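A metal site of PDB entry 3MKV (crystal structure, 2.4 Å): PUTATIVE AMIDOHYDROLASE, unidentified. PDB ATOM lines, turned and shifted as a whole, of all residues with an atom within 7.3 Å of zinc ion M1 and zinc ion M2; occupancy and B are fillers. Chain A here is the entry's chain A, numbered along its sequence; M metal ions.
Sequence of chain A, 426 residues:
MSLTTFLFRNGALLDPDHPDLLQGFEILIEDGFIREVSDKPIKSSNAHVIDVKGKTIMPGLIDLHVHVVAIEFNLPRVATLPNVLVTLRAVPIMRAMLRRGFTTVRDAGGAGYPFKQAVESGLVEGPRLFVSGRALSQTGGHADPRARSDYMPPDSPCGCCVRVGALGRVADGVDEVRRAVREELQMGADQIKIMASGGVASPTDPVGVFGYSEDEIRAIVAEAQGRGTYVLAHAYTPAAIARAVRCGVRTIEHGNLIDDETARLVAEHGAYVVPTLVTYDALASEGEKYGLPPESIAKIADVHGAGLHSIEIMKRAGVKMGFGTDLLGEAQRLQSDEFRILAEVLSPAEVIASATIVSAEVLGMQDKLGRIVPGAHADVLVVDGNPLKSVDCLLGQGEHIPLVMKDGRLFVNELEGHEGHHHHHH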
ATOM      1  N   HIS A  65      -9.178  34.564  31.014  1.00  0.00           N
ATOM      2  CA  HIS A  65      -9.303  33.111  31.120  1.00  0.00           C
ATOM      3  C   HIS A  65      -7.967  32.395  31.089  1.00  0.00           C
ATOM      4  O   HIS A  65      -7.497  31.958  30.055  1.00  0.00           O
ATOM      5  CB  HIS A  65     -10.235  32.548  30.024  1.00  0.00           C
ATOM      6  CG  HIS A  65     -10.743  31.173  30.319  1.00  0.00           C
ATOM      7  ND1 HIS A  65     -12.084  30.893  30.409  1.00  0.00           N
ATOM      8  CD2 HIS A  65     -10.100  30.018  30.564  1.00  0.00           C
ATOM      9  CE1 HIS A  65     -12.244  29.606  30.697  1.00  0.00           C
ATOM     10  NE2 HIS A  65     -11.052  29.064  30.797  1.00  0.00           N
ATOM     11  N   VAL A  66      -7.344  32.267  32.247  1.00  0.00           N
ATOM     12  CA  VAL A  66      -6.130  31.479  32.354  1.00  0.00           C
ATOM     13  C   VAL A  66      -6.304  30.410  33.415  1.00  0.00           C
ATOM     14  O   VAL A  66      -7.215  30.481  34.245  1.00  0.00           O
ATOM     15  CB  VAL A  66      -4.880  32.363  32.699  1.00  0.00           C
ATOM     16  CG1 VAL A  66      -4.682  33.445  31.659  1.00  0.00           C
ATOM     17  CG2 VAL A  66      -5.025  32.995  34.065  1.00  0.00           C
ATOM     18  N   HIS A  67      -5.432  29.414  33.371  1.00  0.00           N
ATOM     19  CA  HIS A  67      -5.282  28.467  34.469  1.00  0.00           C
ATOM     20  C   HIS A  67      -3.818  28.451  34.883  1.00  0.00           C
ATOM     21  O   HIS A  67      -2.968  27.886  34.209  1.00  0.00           O
ATOM     22  CB  HIS A  67      -5.755  27.086  34.051  1.00  0.00           C
ATOM     23  CG  HIS A  67      -7.198  27.051  33.654  1.00  0.00           C
ATOM     24  ND1 HIS A  67      -8.224  27.077  34.569  1.00  0.00           N
ATOM     25  CD2 HIS A  67      -7.782  27.009  32.436  1.00  0.00           C
ATOM     26  CE1 HIS A  67      -9.378  27.041  33.935  1.00  0.00           C
ATOM     27  NE2 HIS A  67      -9.140  27.001  32.638  1.00  0.00           N
ATOM     28  N   ALA A 108      -9.635  30.995  35.632  1.00  0.00           N
ATOM     29  CA  ALA A 108     -10.923  30.380  35.378  1.00  0.00           C
ATOM     30  C   ALA A 108     -11.110  29.058  36.120  1.00  0.00           C
ATOM     31  O   ALA A 108     -12.136  28.400  35.974  1.00  0.00           O
ATOM     32  CB  ALA A 108     -11.115  30.196  33.876  1.00  0.00           C
ATOM     33  N   GLY A 109     -10.124  28.665  36.924  1.00  0.00           N
ATOM     34  CA  GLY A 109     -10.243  27.448  37.702  1.00  0.00           C
ATOM     35  C   GLY A 109      -8.897  26.909  38.128  1.00  0.00           C
ATOM     36  O   GLY A 109      -8.003  26.682  37.292  1.00  0.00           O
ATOM     37  N   HIS A 142     -17.426  18.392  32.628  1.00  0.00           N
ATOM     38  CA  HIS A 142     -16.111  18.821  32.187  1.00  0.00           C
ATOM     39  C   HIS A 142     -15.069  18.641  33.287  1.00  0.00           C
ATOM     40  O   HIS A 142     -14.063  17.970  33.101  1.00  0.00           O
ATOM     41  CB  HIS A 142     -16.144  20.282  31.734  1.00  0.00           C
ATOM     42  CG  HIS A 142     -15.025  20.661  30.817  1.00  0.00           C
ATOM     43  ND1 HIS A 142     -14.792  20.005  29.622  1.00  0.00           N
ATOM     44  CD2 HIS A 142     -14.087  21.631  30.903  1.00  0.00           C
ATOM     45  CE1 HIS A 142     -13.755  20.556  29.023  1.00  0.00           C
ATOM     46  NE2 HIS A 142     -13.299  21.535  29.782  1.00  0.00           N
ATOM     47  N   LEU A 167      -8.217  21.834  39.175  1.00  0.00           N
ATOM     48  CA  LEU A 167      -8.887  22.952  38.518  1.00  0.00           C
ATOM     49  C   LEU A 167     -10.386  23.055  38.889  1.00  0.00           C
ATOM     50  O   LEU A 167     -10.984  24.141  38.837  1.00  0.00           O
ATOM     51  CB  LEU A 167      -8.769  22.838  36.996  1.00  0.00           C
ATOM     52  CG  LEU A 167      -7.439  22.809  36.230  1.00  0.00           C
ATOM     53  CD1 LEU A 167      -7.721  23.214  34.771  1.00  0.00           C
ATOM     54  CD2 LEU A 167      -6.338  23.693  36.814  1.00  0.00           C
ATOM     55  N   KCX A 193     -16.820  29.948  38.932  1.00  0.00           N
ATOM     56  CA  KCX A 193     -16.778  29.224  37.677  1.00  0.00           C
ATOM     57  CB  KCX A 193     -15.349  28.818  37.351  1.00  0.00           C
ATOM     58  CG  KCX A 193     -15.178  27.997  36.056  1.00  0.00           C
ATOM     59  CD  KCX A 193     -15.561  28.835  34.838  1.00  0.00           C
ATOM     60  CE  KCX A 193     -15.212  28.136  33.537  1.00  0.00           C
ATOM     61  NZ  KCX A 193     -13.840  27.574  33.605  1.00  0.00           N
ATOM     62  C   KCX A 193     -17.651  27.967  37.716  1.00  0.00           C
ATOM     63  O   KCX A 193     -17.646  27.221  38.700  1.00  0.00           O
ATOM     64  CX  KCX A 193     -13.271  27.113  32.491  1.00  0.00           C
ATOM     65  OQ1 KCX A 193     -13.883  27.157  31.413  1.00  0.00           O
ATOM     66  OQ2 KCX A 193     -12.128  26.652  32.549  1.00  0.00           O
ATOM     67  N   ILE A 194     -18.369  27.707  36.629  1.00  0.00           N
ATOM     68  CA  ILE A 194     -19.051  26.426  36.465  1.00  0.00           C
ATOM     69  C   ILE A 194     -18.802  25.912  35.066  1.00  0.00           C
ATOM     70  O   ILE A 194     -18.590  26.705  34.137  1.00  0.00           O
ATOM     71  CB  ILE A 194     -20.586  26.561  36.628  1.00  0.00           C
ATOM     72  CG1 ILE A 194     -21.182  27.369  35.464  1.00  0.00           C
ATOM     73  CG2 ILE A 194     -20.921  27.170  37.969  1.00  0.00           C
ATOM     74  CD1 ILE A 194     -22.699  27.283  35.318  1.00  0.00           C
ATOM     75  N   MET A 195     -18.821  24.595  34.925  1.00  0.00           N
ATOM     76  CA  MET A 195     -18.888  23.985  33.608  1.00  0.00           C
ATOM     77  C   MET A 195     -20.357  23.866  33.237  1.00  0.00           C
ATOM     78  O   MET A 195     -21.127  23.158  33.896  1.00  0.00           O
ATOM     79  CB  MET A 195     -18.201  22.613  33.606  1.00  0.00           C
ATOM     80  CG  MET A 195     -16.742  22.643  34.036  1.00  0.00           C
ATOM     81  SD  MET A 195     -15.761  23.999  33.361  1.00  0.00           S
ATOM     82  CE  MET A 195     -14.157  23.588  34.019  1.00  0.00           C
ATOM     83  N   GLY A 198     -20.109  20.175  28.112  1.00  0.00           N
ATOM     84  CA  GLY A 198     -18.978  19.292  27.909  1.00  0.00           C
ATOM     85  C   GLY A 198     -17.811  20.073  27.329  1.00  0.00           C
ATOM     86  O   GLY A 198     -17.959  21.214  26.887  1.00  0.00           O
ATOM     87  N   GLY A 199     -16.636  19.456  27.334  1.00  0.00           N
ATOM     88  CA  GLY A 199     -15.432  20.123  26.879  1.00  0.00           C
ATOM     89  C   GLY A 199     -14.486  19.183  26.171  1.00  0.00           C
ATOM     90  O   GLY A 199     -14.753  17.988  26.066  1.00  0.00           O
ATOM     91  N   ALA A 233     -19.235  30.830  32.968  1.00  0.00           N
ATOM     92  CA  ALA A 233     -19.622  29.474  32.636  1.00  0.00           C
ATOM     93  C   ALA A 233     -19.010  29.038  31.342  1.00  0.00           C
ATOM     94  O   ALA A 233     -19.130  29.732  30.343  1.00  0.00           O
ATOM     95  CB  ALA A 233     -21.134  29.369  32.562  1.00  0.00           C
ATOM     96  N   HIS A 234     -18.368  27.890  31.364  1.00  0.00           N
ATOM     97  CA  HIS A 234     -17.822  27.261  30.174  1.00  0.00           C
ATOM     98  C   HIS A 234     -19.011  26.649  29.414  1.00  0.00           C
ATOM     99  O   HIS A 234     -19.792  25.886  29.986  1.00  0.00           O
ATOM    100  CB  HIS A 234     -16.779  26.229  30.623  1.00  0.00           C
ATOM    101  CG  HIS A 234     -16.543  25.102  29.658  1.00  0.00           C
ATOM    102  ND1 HIS A 234     -15.308  24.864  29.086  1.00  0.00           N
ATOM    103  CD2 HIS A 234     -17.348  24.110  29.223  1.00  0.00           C
ATOM    104  CE1 HIS A 234     -15.372  23.804  28.309  1.00  0.00           C
ATOM    105  NE2 HIS A 234     -16.603  23.327  28.369  1.00  0.00           N
ATOM    106  N   ALA A 235     -19.172  27.039  28.149  1.00  0.00           N
ATOM    107  CA  ALA A 235     -20.298  26.591  27.307  1.00  0.00           C
ATOM    108  C   ALA A 235     -19.983  26.746  25.826  1.00  0.00           C
ATOM    109  O   ALA A 235     -19.516  27.804  25.398  1.00  0.00           O
ATOM    110  CB  ALA A 235     -21.569  27.356  27.661  1.00  0.00           C
ATOM    111  N   TYR A 236     -20.247  25.720  25.028  1.00  0.00           N
ATOM    112  CA  TYR A 236     -19.932  25.749  23.590  1.00  0.00           C
ATOM    113  C   TYR A 236     -21.127  25.979  22.653  1.00  0.00           C
ATOM    114  O   TYR A 236     -21.059  26.831  21.756  1.00  0.00           O
ATOM    115  CB  TYR A 236     -19.190  24.489  23.168  1.00  0.00           C
ATOM    116  CG  TYR A 236     -17.739  24.447  23.604  1.00  0.00           C
ATOM    117  CD1 TYR A 236     -16.872  25.483  23.274  1.00  0.00           C
ATOM    118  CD2 TYR A 236     -17.234  23.365  24.303  1.00  0.00           C
ATOM    119  CE1 TYR A 236     -15.539  25.452  23.658  1.00  0.00           C
ATOM    120  CE2 TYR A 236     -15.909  23.317  24.698  1.00  0.00           C
ATOM    121  CZ  TYR A 236     -15.058  24.370  24.375  1.00  0.00           C
ATOM    122  OH  TYR A 236     -13.738  24.334  24.759  1.00  0.00           O
ATOM    123  N   GLU A 253     -17.786  31.444  28.423  1.00  0.00           N
ATOM    124  CA  GLU A 253     -16.411  31.146  28.092  1.00  0.00           C
ATOM    125  C   GLU A 253     -16.347  30.283  26.832  1.00  0.00           C
ATOM    126  O   GLU A 253     -17.009  29.246  26.737  1.00  0.00           O
ATOM    127  CB  GLU A 253     -15.706  30.457  29.263  1.00  0.00           C
ATOM    128  CG  GLU A 253     -15.817  31.192  30.592  1.00  0.00           C
ATOM    129  CD  GLU A 253     -15.262  32.608  30.559  1.00  0.00           C
ATOM    130  OE1 GLU A 253     -14.050  32.777  30.297  1.00  0.00           O
ATOM    131  OE2 GLU A 253     -16.048  33.562  30.816  1.00  0.00           O
ATOM    132  N   HIS A 254     -15.539  30.740  25.879  1.00  0.00           N
ATOM    133  CA  HIS A 254     -15.359  30.036  24.614  1.00  0.00           C
ATOM    134  C   HIS A 254     -16.477  30.428  23.648  1.00  0.00           C
ATOM    135  O   HIS A 254     -16.278  31.295  22.791  1.00  0.00           O
ATOM    136  CB  HIS A 254     -15.307  28.520  24.833  1.00  0.00           C
ATOM    137  CG  HIS A 254     -14.329  28.104  25.890  1.00  0.00           C
ATOM    138  ND1 HIS A 254     -12.999  28.458  25.862  1.00  0.00           N
ATOM    139  CD2 HIS A 254     -14.489  27.334  26.993  1.00  0.00           C
ATOM    140  CE1 HIS A 254     -12.385  27.937  26.907  1.00  0.00           C
ATOM    141  NE2 HIS A 254     -13.269  27.256  27.604  1.00  0.00           N
ATOM    142  N   THR A 276     -11.517  31.847  23.402  1.00  0.00           N
ATOM    143  CA  THR A 276     -10.173  31.424  23.776  1.00  0.00           C
ATOM    144  C   THR A 276      -9.506  30.653  22.642  1.00  0.00           C
ATOM    145  O   THR A 276      -9.003  29.539  22.839  1.00  0.00           O
ATOM    146  CB  THR A 276     -10.196  30.603  25.088  1.00  0.00           C
ATOM    147  OG1 THR A 276     -11.016  29.440  24.920  1.00  0.00           O
ATOM    148  CG2 THR A 276     -10.759  31.451  26.233  1.00  0.00           C
ATOM    149  N   TYR A 280      -7.171  26.228  21.096  1.00  0.00           N
ATOM    150  CA  TYR A 280      -7.561  25.168  20.160  1.00  0.00           C
ATOM    151  C   TYR A 280      -6.494  24.923  19.099  1.00  0.00           C
ATOM    152  O   TYR A 280      -6.180  23.765  18.790  1.00  0.00           O
ATOM    153  CB  TYR A 280      -8.934  25.470  19.563  1.00  0.00           C
ATOM    154  CG  TYR A 280      -9.924  25.784  20.654  1.00  0.00           C
ATOM    155  CD1 TYR A 280     -10.175  24.861  21.663  1.00  0.00           C
ATOM    156  CD2 TYR A 280     -10.589  27.012  20.713  1.00  0.00           C
ATOM    157  CE1 TYR A 280     -11.053  25.137  22.687  1.00  0.00           C
ATOM    158  CE2 TYR A 280     -11.477  27.292  21.746  1.00  0.00           C
ATOM    159  CZ  TYR A 280     -11.705  26.337  22.730  1.00  0.00           C
ATOM    160  OH  TYR A 280     -12.567  26.576  23.779  1.00  0.00           O
ATOM    161  N   THR A 325      -7.358  33.228  26.761  1.00  0.00           N
ATOM    162  CA  THR A 325      -6.423  32.328  26.097  1.00  0.00           C
ATOM    163  C   THR A 325      -6.685  30.847  26.425  1.00  0.00           C
ATOM    164  O   THR A 325      -6.746  30.024  25.504  1.00  0.00           O
ATOM    165  CB  THR A 325      -4.942  32.729  26.380  1.00  0.00           C
ATOM    166  OG1 THR A 325      -4.689  32.710  27.797  1.00  0.00           O
ATOM    167  CG2 THR A 325      -4.628  34.130  25.823  1.00  0.00           C
ATOM    168  N   ASP A 326      -6.802  30.525  27.708  1.00  0.00           N
ATOM    169  CA  ASP A 326      -7.111  29.158  28.162  1.00  0.00           C
ATOM    170  C   ASP A 326      -6.079  28.116  27.743  1.00  0.00           C
ATOM    171  O   ASP A 326      -6.428  27.018  27.298  1.00  0.00           O
ATOM    172  CB  ASP A 326      -8.504  28.719  27.668  1.00  0.00           C
ATOM    173  CG  ASP A 326      -9.015  27.470  28.364  1.00  0.00           C
ATOM    174  OD1 ASP A 326      -8.563  27.170  29.494  1.00  0.00           O
ATOM    175  OD2 ASP A 326      -9.875  26.759  27.774  1.00  0.00           O
ATOM    176  N   LEU A 327      -4.798  28.437  27.906  1.00  0.00           N
ATOM    177  CA  LEU A 327      -3.716  27.548  27.476  1.00  0.00           C
ATOM    178  C   LEU A 327      -3.221  26.605  28.594  1.00  0.00           C
ATOM    179  O   LEU A 327      -3.346  26.926  29.782  1.00  0.00           O
ATOM    180  CB  LEU A 327      -2.554  28.375  26.911  1.00  0.00           C
ATOM    181  CG  LEU A 327      -2.817  29.093  25.574  1.00  0.00           C
ATOM    182  CD1 LEU A 327      -1.898  30.278  25.375  1.00  0.00           C
ATOM    183  CD2 LEU A 327      -2.718  28.124  24.389  1.00  0.00           C
ATOM    184  N   LEU A 328      -2.638  25.475  28.205  1.00  0.00           N
ATOM    185  CA  LEU A 328      -2.198  24.445  29.146  1.00  0.00           C
ATOM    186  C   LEU A 328      -0.714  24.126  28.997  1.00  0.00           C
ATOM    187  O   LEU A 328      -0.152  24.242  27.915  1.00  0.00           O
ATOM    188  CB  LEU A 328      -3.000  23.156  28.962  1.00  0.00           C
ATOM    189  CG  LEU A 328      -4.520  23.275  28.794  1.00  0.00           C
ATOM    190  CD1 LEU A 328      -5.121  21.936  28.402  1.00  0.00           C
ATOM    191  CD2 LEU A 328      -5.199  23.811  30.062  1.00  0.00           C
HETATM  192 ZN    ZN M   1     -10.421  27.112  31.000  1.00  0.00          ZN
HETATM  193 ZN    ZN M   2     -13.248  25.972  29.693  1.00  0.00          ZN
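Of the 24 residues printed, 5 come within 4 Å of zinc ion M2. The nearest printed residue that does not touch zinc ion M2 is His 142 (4.4 Å).
ND1 of His 65 lies within hydrogen-bond range of OE1 of Glu 253, at 2.7 Å. ND1 of His 67 sits at hydrogen-bond distance from O of Gly 109 (2.8 Å). NZ of KCX 193 lies within hydrogen-bond range of O of Ala 108 (3.0 Å). OD2 of Asp 326 sits close to NE2 of His 254, 3.4 Å away. N of His 234 lies within hydrogen-bond range of O of Ile 194 (3.0 Å). NE2 of His 234 is in hydrogen-bond range of O of Gly 198 (2.9 Å). ND1 of His 254 lies within hydrogen-bond range of OH of Tyr 280. OG1 of Thr 276 sits at hydrogen-bond distance from ND1 of His 254, 2.4 Å away.
OQ1 of KCX 193 is bound to zinc ion M2 (2.2 Å). Zinc ion M2 is bound by ND1 of His 234 (2.4 Å). NE2 of His 254 is bound to zinc ion M2 (2.5 Å). Zinc ion M2 has three donor atoms within binding distance.
Of the 24 residues printed, 4 come within 4 Å of zinc ion M1.
Zinc ion M1 is bound by NE2 of His 65 (2.1 Å), NE2 of His 67 (2.1 Å), OQ2 of KCX 193 (2.4 Å) and OD1 of Asp 326 (2.4 Å). Zinc ion M1 has four donor atoms within binding distance.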
